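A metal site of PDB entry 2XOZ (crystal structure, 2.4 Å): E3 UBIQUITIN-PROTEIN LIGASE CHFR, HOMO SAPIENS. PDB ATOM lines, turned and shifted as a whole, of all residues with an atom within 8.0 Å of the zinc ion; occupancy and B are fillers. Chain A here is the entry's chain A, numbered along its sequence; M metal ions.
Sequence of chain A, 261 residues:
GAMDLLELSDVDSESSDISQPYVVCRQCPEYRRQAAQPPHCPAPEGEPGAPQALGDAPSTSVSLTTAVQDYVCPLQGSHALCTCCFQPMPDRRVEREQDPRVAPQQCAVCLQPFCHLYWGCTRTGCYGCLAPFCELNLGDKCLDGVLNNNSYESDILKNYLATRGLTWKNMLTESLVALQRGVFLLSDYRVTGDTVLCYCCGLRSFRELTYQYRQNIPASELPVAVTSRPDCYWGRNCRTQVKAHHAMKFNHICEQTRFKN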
ATOM      1  N   THR A  83      11.181 -17.538  11.463  1.00  0.00           N
ATOM      2  CA  THR A  83      12.451 -18.251  11.507  1.00  0.00           C
ATOM      3  C   THR A  83      12.263 -19.767  11.686  1.00  0.00           C
ATOM      4  O   THR A  83      13.144 -20.572  11.356  1.00  0.00           O
ATOM      5  CB  THR A  83      13.331 -17.699  12.656  1.00  0.00           C
ATOM      6  OG1 THR A  83      13.483 -16.292  12.498  1.00  0.00           O
ATOM      7  CG2 THR A  83      14.711 -18.369  12.701  1.00  0.00           C
ATOM      8  N   GLN A 106       9.029 -11.418  17.583  1.00  0.00           N
ATOM      9  CA  GLN A 106      10.449 -11.784  17.631  1.00  0.00           C
ATOM     10  C   GLN A 106      10.908 -12.270  19.012  1.00  0.00           C
ATOM     11  O   GLN A 106      10.305 -11.942  20.038  1.00  0.00           O
ATOM     12  CB  GLN A 106      11.355 -10.630  17.155  1.00  0.00           C
ATOM     13  CG  GLN A 106      11.366  -9.394  18.076  1.00  0.00           C
ATOM     14  CD  GLN A 106      12.373  -8.337  17.644  1.00  0.00           C
ATOM     15  OE1 GLN A 106      12.710  -8.209  16.460  1.00  0.00           O
ATOM     16  NE2 GLN A 106      12.862  -7.576  18.613  1.00  0.00           N
ATOM     17  N   CYS A 107      11.988 -13.045  19.014  1.00  0.00           N
ATOM     18  CA  CYS A 107      12.703 -13.415  20.221  1.00  0.00           C
ATOM     19  C   CYS A 107      13.434 -12.192  20.785  1.00  0.00           C
ATOM     20  O   CYS A 107      14.116 -11.487  20.047  1.00  0.00           O
ATOM     21  CB  CYS A 107      13.727 -14.509  19.911  1.00  0.00           C
ATOM     22  SG  CYS A 107      14.705 -15.003  21.323  1.00  0.00           S
ATOM     23  N   ALA A 108      13.267 -11.932  22.073  1.00  0.00           N
ATOM     24  CA  ALA A 108      13.869 -10.763  22.684  1.00  0.00           C
ATOM     25  C   ALA A 108      15.349 -10.955  22.981  1.00  0.00           C
ATOM     26  O   ALA A 108      16.028 -10.015  23.374  1.00  0.00           O
ATOM     27  CB  ALA A 108      13.117 -10.358  23.940  1.00  0.00           C
ATOM     28  N   VAL A 109      15.841 -12.174  22.793  1.00  0.00           N
ATOM     29  CA  VAL A 109      17.261 -12.470  22.932  1.00  0.00           C
ATOM     30  C   VAL A 109      17.989 -12.398  21.581  1.00  0.00           C
ATOM     31  O   VAL A 109      18.964 -11.663  21.434  1.00  0.00           O
ATOM     32  CB  VAL A 109      17.514 -13.872  23.533  1.00  0.00           C
ATOM     33  CG1 VAL A 109      19.013 -14.227  23.474  1.00  0.00           C
ATOM     34  CG2 VAL A 109      16.967 -13.975  24.975  1.00  0.00           C
ATOM     35  N   CYS A 110      17.533 -13.176  20.609  1.00  0.00           N
ATOM     36  CA  CYS A 110      18.271 -13.279  19.344  1.00  0.00           C
ATOM     37  C   CYS A 110      17.698 -12.329  18.281  1.00  0.00           C
ATOM     38  O   CYS A 110      18.298 -12.116  17.239  1.00  0.00           O
ATOM     39  CB  CYS A 110      18.263 -14.722  18.832  1.00  0.00           C
ATOM     40  SG  CYS A 110      16.646 -15.306  18.248  1.00  0.00           S
ATOM     41  N   LEU A 111      16.523 -11.770  18.579  1.00  0.00           N
ATOM     42  CA  LEU A 111      15.879 -10.756  17.743  1.00  0.00           C
ATOM     43  C   LEU A 111      15.422 -11.249  16.362  1.00  0.00           C
ATOM     44  O   LEU A 111      15.016 -10.440  15.522  1.00  0.00           O
ATOM     45  CB  LEU A 111      16.755  -9.521  17.619  1.00  0.00           C
ATOM     46  CG  LEU A 111      17.376  -9.029  18.927  1.00  0.00           C
ATOM     47  CD1 LEU A 111      18.327  -7.866  18.703  1.00  0.00           C
ATOM     48  CD2 LEU A 111      16.331  -8.662  19.956  1.00  0.00           C
ATOM     49  N   GLN A 112      15.461 -12.561  16.118  1.00  0.00           N
ATOM     50  CA  GLN A 112      14.875 -13.126  14.904  1.00  0.00           C
ATOM     51  C   GLN A 112      13.337 -13.189  14.986  1.00  0.00           C
ATOM     52  O   GLN A 112      12.778 -13.182  16.075  1.00  0.00           O
ATOM     53  CB  GLN A 112      15.442 -14.507  14.620  1.00  0.00           C
ATOM     54  CG  GLN A 112      16.944 -14.510  14.443  1.00  0.00           C
ATOM     55  CD  GLN A 112      17.415 -13.335  13.591  1.00  0.00           C
ATOM     56  OE1 GLN A 112      16.943 -13.156  12.461  1.00  0.00           O
ATOM     57  NE2 GLN A 112      18.337 -12.534  14.116  1.00  0.00           N
ATOM     58  N   PRO A 113      12.652 -13.233  13.830  1.00  0.00           N
ATOM     59  CA  PRO A 113      11.181 -13.251  13.906  1.00  0.00           C
ATOM     60  C   PRO A 113      10.577 -14.656  13.972  1.00  0.00           C
ATOM     61  O   PRO A 113      11.057 -15.583  13.317  1.00  0.00           O
ATOM     62  CB  PRO A 113      10.749 -12.539  12.621  1.00  0.00           C
ATOM     63  CG  PRO A 113      11.878 -12.780  11.651  1.00  0.00           C
ATOM     64  CD  PRO A 113      13.127 -13.074  12.444  1.00  0.00           C
ATOM     65  N   PHE A 114       9.516 -14.786  14.766  1.00  0.00           N
ATOM     66  CA  PHE A 114       8.749 -16.028  14.862  1.00  0.00           C
ATOM     67  C   PHE A 114       7.259 -15.741  14.835  1.00  0.00           C
ATOM     68  O   PHE A 114       6.788 -14.743  15.380  1.00  0.00           O
ATOM     69  CB  PHE A 114       9.138 -16.782  16.125  1.00  0.00           C
ATOM     70  CG  PHE A 114      10.589 -17.189  16.166  1.00  0.00           C
ATOM     71  CD1 PHE A 114      10.960 -18.468  15.809  1.00  0.00           C
ATOM     72  CD2 PHE A 114      11.559 -16.271  16.534  1.00  0.00           C
ATOM     73  CE1 PHE A 114      12.296 -18.838  15.837  1.00  0.00           C
ATOM     74  CE2 PHE A 114      12.895 -16.642  16.561  1.00  0.00           C
ATOM     75  CZ  PHE A 114      13.264 -17.925  16.213  1.00  0.00           C
ATOM     76  N   CYS A 129       7.128 -22.045  19.186  1.00  0.00           N
ATOM     77  CA  CYS A 129       8.488 -21.570  19.020  1.00  0.00           C
ATOM     78  C   CYS A 129       8.787 -20.189  19.590  1.00  0.00           C
ATOM     79  O   CYS A 129       9.897 -19.703  19.474  1.00  0.00           O
ATOM     80  CB  CYS A 129       8.850 -21.580  17.519  1.00  0.00           C
ATOM     81  SG  CYS A 129       7.687 -20.683  16.433  1.00  0.00           S
ATOM     82  N   LEU A 130       7.775 -19.554  20.182  1.00  0.00           N
ATOM     83  CA  LEU A 130       7.938 -18.269  20.855  1.00  0.00           C
ATOM     84  C   LEU A 130       7.014 -18.237  22.051  1.00  0.00           C
ATOM     85  O   LEU A 130       5.828 -18.483  21.940  1.00  0.00           O
ATOM     86  CB  LEU A 130       7.620 -17.099  19.909  1.00  0.00           C
ATOM     87  CG  LEU A 130       8.090 -15.700  20.346  1.00  0.00           C
ATOM     88  CD1 LEU A 130       9.620 -15.590  20.291  1.00  0.00           C
ATOM     89  CD2 LEU A 130       7.419 -14.586  19.506  1.00  0.00           C
ATOM     90  N   ASP A 188      23.081 -15.256  28.924  1.00  0.00           N
ATOM     91  CA  ASP A 188      22.186 -14.176  28.527  1.00  0.00           C
ATOM     92  C   ASP A 188      21.628 -13.607  29.828  1.00  0.00           C
ATOM     93  O   ASP A 188      20.515 -13.932  30.243  1.00  0.00           O
ATOM     94  CB  ASP A 188      21.057 -14.685  27.627  1.00  0.00           C
ATOM     95  CG  ASP A 188      21.560 -15.244  26.285  1.00  0.00           C
ATOM     96  OD1 ASP A 188      22.474 -14.645  25.674  1.00  0.00           O
ATOM     97  OD2 ASP A 188      21.040 -16.292  25.848  1.00  0.00           O
ATOM     98  N   VAL A 196      10.256 -13.023  26.658  1.00  0.00           N
ATOM     99  CA  VAL A 196       9.680 -13.739  25.532  1.00  0.00           C
ATOM    100  C   VAL A 196      10.790 -14.154  24.582  1.00  0.00           C
ATOM    101  O   VAL A 196      11.511 -13.319  24.051  1.00  0.00           O
ATOM    102  CB  VAL A 196       8.641 -12.885  24.778  1.00  0.00           C
ATOM    103  CG1 VAL A 196       8.187 -13.598  23.512  1.00  0.00           C
ATOM    104  CG2 VAL A 196       7.438 -12.623  25.686  1.00  0.00           C
ATOM    105  N   LEU A 197      10.934 -15.462  24.387  1.00  0.00           N
ATOM    106  CA  LEU A 197      12.045 -15.914  23.569  1.00  0.00           C
ATOM    107  C   LEU A 197      11.722 -17.147  22.764  1.00  0.00           C
ATOM    108  O   LEU A 197      10.658 -17.743  22.905  1.00  0.00           O
ATOM    109  CB  LEU A 197      13.304 -16.106  24.427  1.00  0.00           C
ATOM    110  CG  LEU A 197      13.093 -16.783  25.778  1.00  0.00           C
ATOM    111  CD1 LEU A 197      12.625 -18.214  25.571  1.00  0.00           C
ATOM    112  CD2 LEU A 197      14.377 -16.736  26.597  1.00  0.00           C
ATOM    113  N   CYS A 198      12.651 -17.519  21.886  1.00  0.00           N
ATOM    114  CA  CYS A 198      12.400 -18.645  21.006  1.00  0.00           C
ATOM    115  C   CYS A 198      12.805 -19.993  21.613  1.00  0.00           C
ATOM    116  O   CYS A 198      13.514 -20.067  22.619  1.00  0.00           O
ATOM    117  CB  CYS A 198      13.072 -18.427  19.649  1.00  0.00           C
ATOM    118  SG  CYS A 198      14.860 -18.508  19.638  1.00  0.00           S
ATOM    119  N   TYR A 199      12.335 -21.055  20.976  1.00  0.00           N
ATOM    120  CA  TYR A 199      12.735 -22.400  21.358  1.00  0.00           C
ATOM    121  C   TYR A 199      14.247 -22.521  21.574  1.00  0.00           C
ATOM    122  O   TYR A 199      14.709 -23.037  22.593  1.00  0.00           O
ATOM    123  CB  TYR A 199      12.298 -23.396  20.281  1.00  0.00           C
ATOM    124  CG  TYR A 199      12.981 -24.726  20.469  1.00  0.00           C
ATOM    125  CD1 TYR A 199      12.584 -25.577  21.485  1.00  0.00           C
ATOM    126  CD2 TYR A 199      14.039 -25.112  19.657  1.00  0.00           C
ATOM    127  CE1 TYR A 199      13.214 -26.792  21.685  1.00  0.00           C
ATOM    128  CE2 TYR A 199      14.666 -26.339  19.848  1.00  0.00           C
ATOM    129  CZ  TYR A 199      14.245 -27.170  20.872  1.00  0.00           C
ATOM    130  OH  TYR A 199      14.860 -28.386  21.080  1.00  0.00           O
ATOM    131  N   CYS A 200      15.022 -22.064  20.598  1.00  0.00           N
ATOM    132  CA  CYS A 200      16.467 -22.213  20.677  1.00  0.00           C
ATOM    133  C   CYS A 200      17.116 -21.410  21.823  1.00  0.00           C
ATOM    134  O   CYS A 200      17.887 -21.965  22.585  1.00  0.00           O
ATOM    135  CB  CYS A 200      17.123 -21.954  19.318  1.00  0.00           C
ATOM    136  SG  CYS A 200      16.926 -23.360  18.136  1.00  0.00           S
ATOM    137  N   CYS A 201      16.780 -20.122  21.967  1.00  0.00           N
ATOM    138  CA  CYS A 201      17.336 -19.333  23.073  1.00  0.00           C
ATOM    139  C   CYS A 201      16.875 -19.862  24.452  1.00  0.00           C
ATOM    140  O   CYS A 201      17.669 -19.905  25.399  1.00  0.00           O
ATOM    141  CB  CYS A 201      17.031 -17.846  22.893  1.00  0.00           C
ATOM    142  SG  CYS A 201      17.772 -17.099  21.373  1.00  0.00           S
ATOM    143  N   GLY A 202      15.604 -20.271  24.569  1.00  0.00           N
ATOM    144  CA  GLY A 202      15.108 -20.892  25.776  1.00  0.00           C
ATOM    145  C   GLY A 202      15.817 -22.205  26.123  1.00  0.00           C
ATOM    146  O   GLY A 202      16.119 -22.449  27.297  1.00  0.00           O
ATOM    147  N   ARG A 204      18.811 -23.087  25.268  1.00  0.00           N
ATOM    148  CA  ARG A 204      20.158 -22.723  25.639  1.00  0.00           C
ATOM    149  C   ARG A 204      20.279 -22.323  27.120  1.00  0.00           C
ATOM    150  O   ARG A 204      21.181 -22.777  27.815  1.00  0.00           O
ATOM    151  CB  ARG A 204      20.675 -21.615  24.720  1.00  0.00           C
ATOM    152  CG  ARG A 204      22.124 -21.242  24.939  1.00  0.00           C
ATOM    153  CD  ARG A 204      22.606 -20.294  23.856  1.00  0.00           C
ATOM    154  NE  ARG A 204      21.925 -18.996  23.898  1.00  0.00           N
ATOM    155  CZ  ARG A 204      21.196 -18.503  22.894  1.00  0.00           C
ATOM    156  NH1 ARG A 204      21.041 -19.202  21.782  1.00  0.00           N
ATOM    157  NH2 ARG A 204      20.607 -17.310  23.010  1.00  0.00           N
HETATM  158 ZN    ZN M   1      15.995 -16.522  20.095  1.00  0.00          ZN
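The zinc ion is bound by the side-chain sulfur (SG) of Cys 201 (2.3 Å), the side-chain sulfur (SG) of Cys 110 (2.3 Å), the side-chain sulfur (SG) of Cys 198 (2.3 Å) and the side-chain sulfur (SG) of Cys 107 (2.3 Å).
The zinc ion has four donor atoms within binding distance.
The guanidinium group (NH2) of Arg 204 lies close to the side-chain sulfur (SG) of Cys 201 (3.3 Å).
NE2 of Gln 112 is in hydrogen-bond range of O of Cys 110.
The side-chain sulfur (SG) of Cys 198 lies close to the backbone NH (N) of Cys 200.
The side-chain sulfur (SG) of Cys 107 sits close to the backbone NH (N) of Val 109, at 3.4 Å.
O of Gln 112 sits at hydrogen-bond distance from N of Cys 107 (3.0 Å).
Of the 21 residues printed, 4 come within 4 Å of the zinc ion.
The nearest printed residue that does not touch the zinc ion is Val 109 (4.6 Å).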
